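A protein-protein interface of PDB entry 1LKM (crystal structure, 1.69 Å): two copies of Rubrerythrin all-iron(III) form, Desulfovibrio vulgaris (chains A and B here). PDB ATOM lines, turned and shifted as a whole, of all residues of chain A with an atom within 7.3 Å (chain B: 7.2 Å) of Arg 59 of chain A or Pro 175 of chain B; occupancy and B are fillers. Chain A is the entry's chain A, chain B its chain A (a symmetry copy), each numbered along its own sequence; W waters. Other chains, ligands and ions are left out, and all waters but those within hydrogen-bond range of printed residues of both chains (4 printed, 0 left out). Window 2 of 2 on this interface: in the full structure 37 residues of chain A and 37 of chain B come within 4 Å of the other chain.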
ATOM      1  N   ILE A  13     -12.374 -35.794 -39.931  1.00  0.00           N
ATOM      2  CA  ILE A  13     -12.665 -34.534 -39.254  1.00  0.00           C
ATOM      3  C   ILE A  13     -14.108 -34.133 -39.552  1.00  0.00           C
ATOM      4  O   ILE A  13     -14.860 -33.782 -38.645  1.00  0.00           O
ATOM      5  CB  ILE A  13     -11.705 -33.407 -39.718  1.00  0.00           C
ATOM      6  CG1 ILE A  13     -10.290 -33.696 -39.208  1.00  0.00           C
ATOM      7  CG2 ILE A  13     -12.199 -32.043 -39.207  1.00  0.00           C
ATOM      8  CD1 ILE A  13      -9.234 -32.733 -39.734  1.00  0.00           C
ATOM      9  N   PHE A  17     -17.218 -33.816 -37.022  1.00  0.00           N
ATOM     10  CA  PHE A  17     -17.971 -32.568 -36.963  1.00  0.00           C
ATOM     11  C   PHE A  17     -19.466 -32.829 -37.132  1.00  0.00           C
ATOM     12  O   PHE A  17     -20.287 -32.224 -36.445  1.00  0.00           O
ATOM     13  CB  PHE A  17     -17.499 -31.599 -38.048  1.00  0.00           C
ATOM     14  CG  PHE A  17     -18.268 -30.310 -38.075  1.00  0.00           C
ATOM     15  CD1 PHE A  17     -18.125 -29.378 -37.053  1.00  0.00           C
ATOM     16  CD2 PHE A  17     -19.163 -30.043 -39.105  1.00  0.00           C
ATOM     17  CE1 PHE A  17     -18.865 -28.194 -37.055  1.00  0.00           C
ATOM     18  CE2 PHE A  17     -19.907 -28.866 -39.115  1.00  0.00           C
ATOM     19  CZ  PHE A  17     -19.758 -27.939 -38.089  1.00  0.00           C
ATOM     20  N   GLU A  53     -20.029 -29.735 -26.795  1.00  0.00           N
ATOM     21  CA  GLU A  53     -19.955 -30.440 -28.077  1.00  0.00           C
ATOM     22  C   GLU A  53     -19.825 -29.382 -29.176  1.00  0.00           C
ATOM     23  O   GLU A  53     -19.191 -29.619 -30.205  1.00  0.00           O
ATOM     24  CB  GLU A  53     -21.208 -31.280 -28.340  1.00  0.00           C
ATOM     25  CG  GLU A  53     -21.492 -32.378 -27.327  1.00  0.00           C
ATOM     26  CD  GLU A  53     -20.302 -33.280 -27.051  1.00  0.00           C
ATOM     27  OE1 GLU A  53     -19.498 -33.528 -27.974  1.00  0.00           O
ATOM     28  OE2 GLU A  53     -20.185 -33.756 -25.903  1.00  0.00           O
ATOM     29  N   ARG A  54     -20.443 -28.224 -28.958  1.00  0.00           N
ATOM     30  CA  ARG A  54     -20.373 -27.127 -29.920  1.00  0.00           C
ATOM     31  C   ARG A  54     -18.915 -26.702 -30.072  1.00  0.00           C
ATOM     32  O   ARG A  54     -18.455 -26.403 -31.174  1.00  0.00           O
ATOM     33  CB  ARG A  54     -21.194 -25.932 -29.427  1.00  0.00           C
ATOM     34  CG  ARG A  54     -21.054 -24.667 -30.274  1.00  0.00           C
ATOM     35  CD  ARG A  54     -21.597 -23.461 -29.509  1.00  0.00           C
ATOM     36  NE  ARG A  54     -20.825 -23.240 -28.292  1.00  0.00           N
ATOM     37  CZ  ARG A  54     -21.262 -22.581 -27.225  1.00  0.00           C
ATOM     38  NH1 ARG A  54     -22.482 -22.063 -27.208  1.00  0.00           N
ATOM     39  NH2 ARG A  54     -20.476 -22.456 -26.163  1.00  0.00           N
ATOM     40  N   GLU A  55     -18.193 -26.690 -28.956  1.00  0.00           N
ATOM     41  CA  GLU A  55     -16.791 -26.290 -28.959  1.00  0.00           C
ATOM     42  C   GLU A  55     -15.874 -27.355 -29.566  1.00  0.00           C
ATOM     43  O   GLU A  55     -14.906 -27.023 -30.246  1.00  0.00           O
ATOM     44  CB  GLU A  55     -16.363 -25.924 -27.537  1.00  0.00           C
ATOM     45  CG  GLU A  55     -17.114 -24.704 -26.987  1.00  0.00           C
ATOM     46  CD  GLU A  55     -16.931 -23.472 -27.861  1.00  0.00           C
ATOM     47  OE1 GLU A  55     -15.772 -23.157 -28.199  1.00  0.00           O
ATOM     48  OE2 GLU A  55     -17.939 -22.816 -28.205  1.00  0.00           O
ATOM     49  N   HIS A  56     -16.166 -28.629 -29.329  1.00  0.00           N
ATOM     50  CA  HIS A  56     -15.356 -29.686 -29.937  1.00  0.00           C
ATOM     51  C   HIS A  56     -15.541 -29.557 -31.449  1.00  0.00           C
ATOM     52  O   HIS A  56     -14.585 -29.642 -32.223  1.00  0.00           O
ATOM     53  CB  HIS A  56     -15.843 -31.066 -29.489  1.00  0.00           C
ATOM     54  CG  HIS A  56     -15.509 -31.391 -28.067  1.00  0.00           C
ATOM     55  ND1 HIS A  56     -16.253 -32.272 -27.311  1.00  0.00           N
ATOM     56  CD2 HIS A  56     -14.519 -30.944 -27.260  1.00  0.00           C
ATOM     57  CE1 HIS A  56     -15.739 -32.347 -26.096  1.00  0.00           C
ATOM     58  NE2 HIS A  56     -14.688 -31.551 -26.038  1.00  0.00           N
ATOM     59  N   ALA A  57     -16.788 -29.341 -31.857  1.00  0.00           N
ATOM     60  CA  ALA A  57     -17.119 -29.199 -33.265  1.00  0.00           C
ATOM     61  C   ALA A  57     -16.420 -27.996 -33.887  1.00  0.00           C
ATOM     62  O   ALA A  57     -15.971 -28.067 -35.028  1.00  0.00           O
ATOM     63  CB  ALA A  57     -18.633 -29.073 -33.439  1.00  0.00           C
ATOM     64  N   LYS A  58     -16.321 -26.899 -33.141  1.00  0.00           N
ATOM     65  CA  LYS A  58     -15.669 -25.701 -33.666  1.00  0.00           C
ATOM     66  C   LYS A  58     -14.186 -25.947 -33.917  1.00  0.00           C
ATOM     67  O   LYS A  58     -13.654 -25.552 -34.955  1.00  0.00           O
ATOM     68  CB  LYS A  58     -15.844 -24.514 -32.712  1.00  0.00           C
ATOM     69  CG  LYS A  58     -15.445 -23.190 -33.351  1.00  0.00           C
ATOM     70  CD  LYS A  58     -15.663 -22.002 -32.429  1.00  0.00           C
ATOM     71  CE  LYS A  58     -15.314 -20.705 -33.147  1.00  0.00           C
ATOM     72  NZ  LYS A  58     -15.504 -19.510 -32.281  1.00  0.00           N
ATOM     73  N   ARG A  59     -13.519 -26.596 -32.967  1.00  0.00           N
ATOM     74  CA  ARG A  59     -12.097 -26.901 -33.117  1.00  0.00           C
ATOM     75  C   ARG A  59     -11.904 -27.752 -34.369  1.00  0.00           C
ATOM     76  O   ARG A  59     -10.991 -27.517 -35.159  1.00  0.00           O
ATOM     77  CB  ARG A  59     -11.572 -27.656 -31.887  1.00  0.00           C
ATOM     78  CG  ARG A  59     -10.057 -27.906 -31.900  1.00  0.00           C
ATOM     79  CD  ARG A  59      -9.296 -26.589 -31.808  1.00  0.00           C
ATOM     80  NE  ARG A  59      -7.870 -26.699 -32.134  1.00  0.00           N
ATOM     81  CZ  ARG A  59      -6.936 -27.168 -31.314  1.00  0.00           C
ATOM     82  NH1 ARG A  59      -7.257 -27.586 -30.096  1.00  0.00           N
ATOM     83  NH2 ARG A  59      -5.667 -27.196 -31.706  1.00  0.00           N
ATOM     84  N   LEU A  60     -12.776 -28.742 -34.547  1.00  0.00           N
ATOM     85  CA  LEU A  60     -12.702 -29.628 -35.703  1.00  0.00           C
ATOM     86  C   LEU A  60     -12.984 -28.869 -36.993  1.00  0.00           C
ATOM     87  O   LEU A  60     -12.267 -29.016 -37.983  1.00  0.00           O
ATOM     88  CB  LEU A  60     -13.709 -30.775 -35.550  1.00  0.00           C
ATOM     89  CG  LEU A  60     -13.454 -31.760 -34.404  1.00  0.00           C
ATOM     90  CD1 LEU A  60     -14.676 -32.651 -34.202  1.00  0.00           C
ATOM     91  CD2 LEU A  60     -12.218 -32.593 -34.715  1.00  0.00           C
ATOM     92  N   PHE A  61     -14.034 -28.054 -36.970  1.00  0.00           N
ATOM     93  CA  PHE A  61     -14.441 -27.271 -38.129  1.00  0.00           C
ATOM     94  C   PHE A  61     -13.321 -26.360 -38.626  1.00  0.00           C
ATOM     95  O   PHE A  61     -13.110 -26.222 -39.830  1.00  0.00           O
ATOM     96  CB  PHE A  61     -15.665 -26.420 -37.773  1.00  0.00           C
ATOM     97  CG  PHE A  61     -16.340 -25.787 -38.961  1.00  0.00           C
ATOM     98  CD1 PHE A  61     -17.071 -26.562 -39.857  1.00  0.00           C
ATOM     99  CD2 PHE A  61     -16.258 -24.416 -39.174  1.00  0.00           C
ATOM    100  CE1 PHE A  61     -17.716 -25.977 -40.950  1.00  0.00           C
ATOM    101  CE2 PHE A  61     -16.901 -23.819 -40.268  1.00  0.00           C
ATOM    102  CZ  PHE A  61     -17.629 -24.601 -41.153  1.00  0.00           C
ATOM    103  N   LYS A  62     -12.599 -25.746 -37.696  1.00  0.00           N
ATOM    104  CA  LYS A  62     -11.525 -24.832 -38.067  1.00  0.00           C
ATOM    105  C   LYS A  62     -10.332 -25.484 -38.760  1.00  0.00           C
ATOM    106  O   LYS A  62      -9.518 -24.791 -39.373  1.00  0.00           O
ATOM    107  CB  LYS A  62     -11.071 -24.040 -36.837  1.00  0.00           C
ATOM    108  CG  LYS A  62     -12.142 -23.074 -36.347  1.00  0.00           C
ATOM    109  CD  LYS A  62     -11.743 -22.330 -35.084  1.00  0.00           C
ATOM    110  CE  LYS A  62     -10.635 -21.327 -35.344  1.00  0.00           C
ATOM    111  NZ  LYS A  62     -10.420 -20.442 -34.167  1.00  0.00           N
ATOM    112  N   PHE A  63     -10.224 -26.807 -38.678  1.00  0.00           N
ATOM    113  CA  PHE A  63      -9.127 -27.511 -39.336  1.00  0.00           C
ATOM    114  C   PHE A  63      -9.395 -27.678 -40.829  1.00  0.00           C
ATOM    115  O   PHE A  63      -8.463 -27.761 -41.630  1.00  0.00           O
ATOM    116  CB  PHE A  63      -8.913 -28.901 -38.725  1.00  0.00           C
ATOM    117  CG  PHE A  63      -8.171 -28.892 -37.416  1.00  0.00           C
ATOM    118  CD1 PHE A  63      -6.950 -28.235 -37.296  1.00  0.00           C
ATOM    119  CD2 PHE A  63      -8.678 -29.569 -36.313  1.00  0.00           C
ATOM    120  CE1 PHE A  63      -6.243 -28.254 -36.093  1.00  0.00           C
ATOM    121  CE2 PHE A  63      -7.980 -29.595 -35.107  1.00  0.00           C
ATOM    122  CZ  PHE A  63      -6.760 -28.935 -34.998  1.00  0.00           C
ATOM    123  N   LEU A  64     -10.670 -27.731 -41.199  1.00  0.00           N
ATOM    124  CA  LEU A  64     -11.051 -27.918 -42.595  1.00  0.00           C
ATOM    125  C   LEU A  64     -10.644 -26.749 -43.485  1.00  0.00           C
ATOM    126  O   LEU A  64     -10.546 -25.612 -43.028  1.00  0.00           O
ATOM    127  CB  LEU A  64     -12.554 -28.186 -42.680  1.00  0.00           C
ATOM    128  CG  LEU A  64     -12.933 -29.462 -41.917  1.00  0.00           C
ATOM    129  CD1 LEU A  64     -14.434 -29.696 -41.969  1.00  0.00           C
ATOM    130  CD2 LEU A  64     -12.185 -30.646 -42.523  1.00  0.00           C
ATOM    131  N   GLU A 116      -0.616 -32.727 -34.912  1.00  0.00           N
ATOM    132  CA  GLU A 116      -1.429 -31.803 -34.128  1.00  0.00           C
ATOM    133  C   GLU A 116      -2.886 -32.247 -34.077  1.00  0.00           C
ATOM    134  O   GLU A 116      -3.490 -32.290 -33.005  1.00  0.00           O
ATOM    135  CB  GLU A 116      -1.353 -30.381 -34.689  1.00  0.00           C
ATOM    136  CG  GLU A 116      -2.177 -29.383 -33.883  1.00  0.00           C
ATOM    137  CD  GLU A 116      -2.049 -27.953 -34.375  1.00  0.00           C
ATOM    138  OE1 GLU A 116      -2.705 -27.066 -33.787  1.00  0.00           O
ATOM    139  OE2 GLU A 116      -1.298 -27.714 -35.344  1.00  0.00           O
ATOM    140  N   ILE A 117      -3.446 -32.575 -35.237  1.00  0.00           N
ATOM    141  CA  ILE A 117      -4.835 -33.012 -35.310  1.00  0.00           C
ATOM    142  C   ILE A 117      -5.044 -34.291 -34.504  1.00  0.00           C
ATOM    143  O   ILE A 117      -6.051 -34.442 -33.809  1.00  0.00           O
ATOM    144  CB  ILE A 117      -5.266 -33.234 -36.782  1.00  0.00           C
ATOM    145  CG1 ILE A 117      -5.294 -31.885 -37.508  1.00  0.00           C
ATOM    146  CG2 ILE A 117      -6.633 -33.912 -36.844  1.00  0.00           C
ATOM    147  CD1 ILE A 117      -5.611 -31.974 -38.985  1.00  0.00           C
ATOM    148  N   ARG A 119      -3.458 -35.233 -31.885  1.00  0.00           N
ATOM    149  CA  ARG A 119      -3.442 -34.892 -30.467  1.00  0.00           C
ATOM    150  C   ARG A 119      -4.765 -34.278 -30.031  1.00  0.00           C
ATOM    151  O   ARG A 119      -5.213 -34.485 -28.902  1.00  0.00           O
ATOM    152  CB  ARG A 119      -2.292 -33.930 -30.157  1.00  0.00           C
ATOM    153  CG  ARG A 119      -0.936 -34.432 -30.634  1.00  0.00           C
ATOM    154  CD  ARG A 119       0.190 -33.982 -29.718  1.00  0.00           C
ATOM    155  NE  ARG A 119       0.094 -34.621 -28.410  1.00  0.00           N
ATOM    156  CZ  ARG A 119       0.997 -34.494 -27.443  1.00  0.00           C
ATOM    157  NH1 ARG A 119       2.076 -33.746 -27.631  1.00  0.00           N
ATOM    158  NH2 ARG A 119       0.821 -35.120 -26.286  1.00  0.00           N
ATOM    159  N   VAL A 120      -5.391 -33.519 -30.926  1.00  0.00           N
ATOM    160  CA  VAL A 120      -6.670 -32.903 -30.607  1.00  0.00           C
ATOM    161  C   VAL A 120      -7.740 -33.985 -30.506  1.00  0.00           C
ATOM    162  O   VAL A 120      -8.579 -33.944 -29.608  1.00  0.00           O
ATOM    163  CB  VAL A 120      -7.085 -31.865 -31.669  1.00  0.00           C
ATOM    164  CG1 VAL A 120      -8.503 -31.377 -31.398  1.00  0.00           C
ATOM    165  CG2 VAL A 120      -6.116 -30.689 -31.642  1.00  0.00           C
ATOM    166  N   PHE A 121      -7.716 -34.948 -31.425  1.00  0.00           N
ATOM    167  CA  PHE A 121      -8.687 -36.040 -31.384  1.00  0.00           C
ATOM    168  C   PHE A 121      -8.564 -36.750 -30.042  1.00  0.00           C
ATOM    169  O   PHE A 121      -9.562 -37.022 -29.370  1.00  0.00           O
ATOM    170  CB  PHE A 121      -8.428 -37.074 -32.487  1.00  0.00           C
ATOM    171  CG  PHE A 121      -8.963 -36.693 -33.842  1.00  0.00           C
ATOM    172  CD1 PHE A 121     -10.215 -36.100 -33.979  1.00  0.00           C
ATOM    173  CD2 PHE A 121      -8.244 -37.006 -34.990  1.00  0.00           C
ATOM    174  CE1 PHE A 121     -10.744 -35.829 -35.239  1.00  0.00           C
ATOM    175  CE2 PHE A 121      -8.765 -36.739 -36.257  1.00  0.00           C
ATOM    176  CZ  PHE A 121     -10.016 -36.152 -36.382  1.00  0.00           C
ATOM    177  N   ALA A 122      -7.326 -37.055 -29.660  1.00  0.00           N
ATOM    178  CA  ALA A 122      -7.064 -37.750 -28.403  1.00  0.00           C
ATOM    179  C   ALA A 122      -7.509 -36.931 -27.197  1.00  0.00           C
ATOM    180  O   ALA A 122      -8.038 -37.476 -26.230  1.00  0.00           O
ATOM    181  CB  ALA A 122      -5.576 -38.074 -28.289  1.00  0.00           C
ATOM    182  N   SER A 123      -7.294 -35.620 -27.261  1.00  0.00           N
ATOM    183  CA  SER A 123      -7.668 -34.738 -26.160  1.00  0.00           C
ATOM    184  C   SER A 123      -9.184 -34.649 -26.016  1.00  0.00           C
ATOM    185  O   SER A 123      -9.709 -34.658 -24.901  1.00  0.00           O
ATOM    186  CB  SER A 123      -7.067 -33.348 -26.373  1.00  0.00           C
ATOM    187  OG  SER A 123      -5.647 -33.403 -26.289  1.00  0.00           O
ATOM    188  N   ILE A 124      -9.888 -34.570 -27.140  1.00  0.00           N
ATOM    189  CA  ILE A 124     -11.341 -34.502 -27.096  1.00  0.00           C
ATOM    190  C   ILE A 124     -11.880 -35.769 -26.438  1.00  0.00           C
ATOM    191  O   ILE A 124     -12.842 -35.717 -25.670  1.00  0.00           O
ATOM    192  CB  ILE A 124     -11.952 -34.359 -28.513  1.00  0.00           C
ATOM    193  CG1 ILE A 124     -11.574 -32.998 -29.107  1.00  0.00           C
ATOM    194  CG2 ILE A 124     -13.472 -34.499 -28.436  1.00  0.00           C
ATOM    195  CD1 ILE A 124     -11.993 -32.806 -30.563  1.00  0.00           C
ATOM    196  N   CYS B 158     -11.867 -28.118 -18.125  1.00  0.00           N
ATOM    197  CA  CYS B 158     -12.028 -26.960 -18.992  1.00  0.00           C
ATOM    198  C   CYS B 158     -13.529 -26.697 -19.066  1.00  0.00           C
ATOM    199  O   CYS B 158     -14.294 -27.571 -19.475  1.00  0.00           O
ATOM    200  CB  CYS B 158     -11.492 -27.259 -20.395  1.00  0.00           C
ATOM    201  SG  CYS B 158     -11.802 -25.924 -21.571  1.00  0.00           S
ATOM    202  N   CYS B 161     -14.915 -26.878 -23.004  1.00  0.00           N
ATOM    203  CA  CYS B 161     -15.133 -28.134 -23.721  1.00  0.00           C
ATOM    204  C   CYS B 161     -15.223 -29.407 -22.883  1.00  0.00           C
ATOM    205  O   CYS B 161     -15.568 -30.467 -23.409  1.00  0.00           O
ATOM    206  CB  CYS B 161     -14.039 -28.321 -24.777  1.00  0.00           C
ATOM    207  SG  CYS B 161     -12.433 -28.825 -24.101  1.00  0.00           S
ATOM    208  N   TYR B 163     -12.615 -30.840 -21.236  1.00  0.00           N
ATOM    209  CA  TYR B 163     -11.349 -31.558 -21.128  1.00  0.00           C
ATOM    210  C   TYR B 163     -10.911 -31.630 -19.664  1.00  0.00           C
ATOM    211  O   TYR B 163     -11.085 -30.675 -18.909  1.00  0.00           O
ATOM    212  CB  TYR B 163     -10.260 -30.859 -21.944  1.00  0.00           C
ATOM    213  CG  TYR B 163      -8.919 -31.545 -21.838  1.00  0.00           C
ATOM    214  CD1 TYR B 163      -8.678 -32.751 -22.494  1.00  0.00           C
ATOM    215  CD2 TYR B 163      -7.907 -31.013 -21.039  1.00  0.00           C
ATOM    216  CE1 TYR B 163      -7.457 -33.417 -22.356  1.00  0.00           C
ATOM    217  CE2 TYR B 163      -6.689 -31.667 -20.891  1.00  0.00           C
ATOM    218  CZ  TYR B 163      -6.469 -32.868 -21.552  1.00  0.00           C
ATOM    219  OH  TYR B 163      -5.263 -33.512 -21.416  1.00  0.00           O
ATOM    220  N   VAL B 164     -10.348 -32.767 -19.269  1.00  0.00           N
ATOM    221  CA  VAL B 164      -9.872 -32.952 -17.901  1.00  0.00           C
ATOM    222  C   VAL B 164      -8.349 -33.063 -17.908  1.00  0.00           C
ATOM    223  O   VAL B 164      -7.780 -33.906 -18.605  1.00  0.00           O
ATOM    224  CB  VAL B 164     -10.472 -34.224 -17.257  1.00  0.00           C
ATOM    225  CG1 VAL B 164      -9.886 -34.427 -15.863  1.00  0.00           C
ATOM    226  CG2 VAL B 164     -11.990 -34.096 -17.172  1.00  0.00           C
ATOM    227  N   HIS B 165      -7.704 -32.195 -17.134  1.00  0.00           N
ATOM    228  CA  HIS B 165      -6.248 -32.160 -17.023  1.00  0.00           C
ATOM    229  C   HIS B 165      -5.824 -32.609 -15.634  1.00  0.00           C
ATOM    230  O   HIS B 165      -6.381 -32.155 -14.634  1.00  0.00           O
ATOM    231  CB  HIS B 165      -5.736 -30.736 -17.257  1.00  0.00           C
ATOM    232  CG  HIS B 165      -4.270 -30.572 -16.995  1.00  0.00           C
ATOM    233  ND1 HIS B 165      -3.304 -31.004 -17.877  1.00  0.00           N
ATOM    234  CD2 HIS B 165      -3.606 -30.051 -15.936  1.00  0.00           C
ATOM    235  CE1 HIS B 165      -2.108 -30.756 -17.373  1.00  0.00           C
ATOM    236  NE2 HIS B 165      -2.263 -30.179 -16.195  1.00  0.00           N
ATOM    237  N   PRO B 171      -3.449 -26.055 -17.390  1.00  0.00           N
ATOM    238  CA  PRO B 171      -2.511 -25.758 -18.477  1.00  0.00           C
ATOM    239  C   PRO B 171      -2.733 -24.359 -19.047  1.00  0.00           C
ATOM    240  O   PRO B 171      -3.805 -23.775 -18.884  1.00  0.00           O
ATOM    241  CB  PRO B 171      -2.818 -26.849 -19.492  1.00  0.00           C
ATOM    242  CG  PRO B 171      -4.311 -26.998 -19.348  1.00  0.00           C
ATOM    243  CD  PRO B 171      -4.499 -26.989 -17.840  1.00  0.00           C
ATOM    244  N   LEU B 173      -2.976 -23.615 -22.107  1.00  0.00           N
ATOM    245  CA  LEU B 173      -3.933 -23.768 -23.197  1.00  0.00           C
ATOM    246  C   LEU B 173      -4.585 -25.139 -23.109  1.00  0.00           C
ATOM    247  O   LEU B 173      -3.917 -26.132 -22.822  1.00  0.00           O
ATOM    248  CB  LEU B 173      -3.232 -23.643 -24.553  1.00  0.00           C
ATOM    249  CG  LEU B 173      -2.695 -22.278 -24.986  1.00  0.00           C
ATOM    250  CD1 LEU B 173      -1.970 -22.420 -26.317  1.00  0.00           C
ATOM    251  CD2 LEU B 173      -3.842 -21.288 -25.113  1.00  0.00           C
ATOM    252  N   CYS B 174      -5.890 -25.199 -23.346  1.00  0.00           N
ATOM    253  CA  CYS B 174      -6.580 -26.481 -23.313  1.00  0.00           C
ATOM    254  C   CYS B 174      -6.129 -27.264 -24.540  1.00  0.00           C
ATOM    255  O   CYS B 174      -6.235 -26.776 -25.665  1.00  0.00           O
ATOM    256  CB  CYS B 174      -8.096 -26.286 -23.367  1.00  0.00           C
ATOM    257  SG  CYS B 174      -9.005 -27.849 -23.430  1.00  0.00           S
ATOM    258  N   PRO B 175      -5.613 -28.488 -24.343  1.00  0.00           N
ATOM    259  CA  PRO B 175      -5.168 -29.272 -25.499  1.00  0.00           C
ATOM    260  C   PRO B 175      -6.297 -29.699 -26.434  1.00  0.00           C
ATOM    261  O   PRO B 175      -6.049 -30.056 -27.585  1.00  0.00           O
ATOM    262  CB  PRO B 175      -4.450 -30.457 -24.858  1.00  0.00           C
ATOM    263  CG  PRO B 175      -5.167 -30.631 -23.569  1.00  0.00           C
ATOM    264  CD  PRO B 175      -5.356 -29.206 -23.083  1.00  0.00           C
ATOM    265  N   ALA B 176      -7.535 -29.656 -25.947  1.00  0.00           N
ATOM    266  CA  ALA B 176      -8.673 -30.039 -26.776  1.00  0.00           C
ATOM    267  C   ALA B 176      -9.258 -28.868 -27.568  1.00  0.00           C
ATOM    268  O   ALA B 176      -9.313 -28.918 -28.798  1.00  0.00           O
ATOM    269  CB  ALA B 176      -9.765 -30.686 -25.916  1.00  0.00           C
ATOM    270  N   CYS B 177      -9.678 -27.807 -26.877  1.00  0.00           N
ATOM    271  CA  CYS B 177     -10.289 -26.660 -27.557  1.00  0.00           C
ATOM    272  C   CYS B 177      -9.407 -25.426 -27.746  1.00  0.00           C
ATOM    273  O   CYS B 177      -9.863 -24.411 -28.272  1.00  0.00           O
ATOM    274  CB  CYS B 177     -11.571 -26.239 -26.829  1.00  0.00           C
ATOM    275  SG  CYS B 177     -11.278 -25.420 -25.248  1.00  0.00           S
ATOM    276  N   ALA B 178      -8.155 -25.510 -27.308  1.00  0.00           N
ATOM    277  CA  ALA B 178      -7.198 -24.418 -27.446  1.00  0.00           C
ATOM    278  C   ALA B 178      -7.557 -23.132 -26.710  1.00  0.00           C
ATOM    279  O   ALA B 178      -6.965 -22.082 -26.969  1.00  0.00           O
ATOM    280  CB  ALA B 178      -6.961 -24.119 -28.930  1.00  0.00           C
ATOM    281  N   HIS B 179      -8.529 -23.189 -25.806  1.00  0.00           N
ATOM    282  CA  HIS B 179      -8.878 -21.989 -25.055  1.00  0.00           C
ATOM    283  C   HIS B 179      -7.876 -21.804 -23.922  1.00  0.00           C
ATOM    284  O   HIS B 179      -7.261 -22.769 -23.463  1.00  0.00           O
ATOM    285  CB  HIS B 179     -10.312 -22.077 -24.526  1.00  0.00           C
ATOM    286  CG  HIS B 179     -11.339 -21.683 -25.540  1.00  0.00           C
ATOM    287  ND1 HIS B 179     -11.439 -22.295 -26.772  1.00  0.00           N
ATOM    288  CD2 HIS B 179     -12.279 -20.710 -25.526  1.00  0.00           C
ATOM    289  CE1 HIS B 179     -12.395 -21.712 -27.473  1.00  0.00           C
ATOM    290  NE2 HIS B 179     -12.920 -20.747 -26.740  1.00  0.00           N
ATOM    291  N   PHE B 184     -10.324 -22.971 -17.009  1.00  0.00           N
ATOM    292  CA  PHE B 184     -10.234 -24.113 -16.105  1.00  0.00           C
ATOM    293  C   PHE B 184     -10.693 -23.903 -14.665  1.00  0.00           C
ATOM    294  O   PHE B 184     -10.611 -22.808 -14.114  1.00  0.00           O
ATOM    295  CB  PHE B 184      -8.805 -24.668 -16.092  1.00  0.00           C
ATOM    296  CG  PHE B 184      -8.442 -25.431 -17.334  1.00  0.00           C
ATOM    297  CD1 PHE B 184      -7.963 -24.770 -18.461  1.00  0.00           C
ATOM    298  CD2 PHE B 184      -8.602 -26.815 -17.383  1.00  0.00           C
ATOM    299  CE1 PHE B 184      -7.646 -25.480 -19.624  1.00  0.00           C
ATOM    300  CE2 PHE B 184      -8.290 -27.535 -18.537  1.00  0.00           C
ATOM    301  CZ  PHE B 184      -7.810 -26.864 -19.661  1.00  0.00           C
HETATM  302  O   HOH W   1      -4.325 -34.499 -23.896  1.00  0.00           O
HETATM  303  O   HOH W   2     -15.411 -20.658 -29.008  1.00  0.00           O
HETATM  304  O   HOH W   3      -3.812 -31.309 -28.381  1.00  0.00           O
HETATM  305  O   HOH W   4      -4.905 -26.784 -28.027  1.00  0.00           O
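NE of Arg 54 of chain A is in salt-bridge range of OE2 of Glu 55 of chain A (2.9 Å).
The side-chain carboxylate (OE1) of Glu 116 of chain A is in salt-bridge range of the guanidinium group (NH2) of Arg 59 of chain A (3.6 Å).
The backbone NH (N) of Cys 158 of chain B lies within hydrogen-bond range of the backbone carbonyl oxygen (O) of Tyr 163 of chain B, 2.8 Å away.
N of Tyr 163 of chain B lies close to SG of Cys 161 of chain B (3.5 Å).
O of His 179 of chain B lies within hydrogen-bond range of N of Cys 174 of chain B, at 2.8 Å.
The backbone carbonyl oxygen (O) of Cys 177 of chain B is in hydrogen-bond range of a ring nitrogen (ND1) of His 179 of chain B, 3.0 Å away.
Of the printed residues of chain B, Glu 55 of chain A touches His 179.
Ile 117 of chain A touches none of the printed residues of chain B.
Of the printed residues of chain A, Tyr 163 of chain B touches Ser 123.
Pro 175 of chain B touches just these residues of chain A: Arg 59 and Ser 123.
Printed residues of chain A within 4 Å of Ala 176 of chain B: Arg 59, Val 120 and Ser 123.
Of the printed residues of chain A, Ala 178 of chain B touches Arg 59 (3.6 Å).
The nearest printed residue of chain A that does not touch His 179 of chain B is Lys 58 of chain A (5.9 Å).
Among the printed residues, merely in contact across the chains: Glu 55 of chain A with His 179 of chain B (3.7 Å), Arg 59 of chain A with Pro 175 of chain B (3.7 Å), Arg 59 of chain A with Cys 177 of chain B (3.8 Å), Arg 59 of chain A with Ala 178 of chain B (3.6 Å), Val 120 of chain A with Ala 176 of chain B (3.7 Å), Ser 123 of chain A with Tyr 163 of chain B (3.2 Å), Ser 123 of chain A with Pro 175 of chain B (3.5 Å) and Ser 123 of chain A with Ala 176 of chain B (3.7 Å).
Hydrophobic or aromatic side chains of chain B that line the printed part of chain A: Tyr 163, Pro 175, Ala 176, Ala 178 and His 179.
Printed residues of chain A that touch a printed residue of chain B: Glu 55, His 56, Arg 59, Val 120 and Ser 123.
Among the printed residues, no Asp or Glu carboxylate lies within 4 Å of a Lys or Arg side-chain nitrogen of the other chain.
NE2 of His 56 of chain A is in hydrogen-bond range of O of Cys 161 of chain B.
NH1 of Arg 59 of chain A sits at hydrogen-bond distance from O of Ala 176 of chain B, 2.8 Å away.
Water W2 lies within hydrogen-bond range of OE1 of Glu 55 of chain A (2.7 Å), NE2 of His 179 of chain B (3.4 Å) and NZ of Lys 58 of chain A (3.5 Å).
Water W3 bridges the backbone carbonyl oxygen of Pro 175 of chain B and the side-chain hydroxyl of Ser 123 of chain A.
Water W4 lies within hydrogen-bond range of O of Cys 174 of chain B (2.7 Å), NH1 of Arg 59 of chain A (3.2 Å) and O of Pro 175 of chain B (3.5 Å).
Water W1 lies within hydrogen-bond range of OH of Tyr 163 of chain B and OG of Ser 123 of chain A.
No position is printed for both chains.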
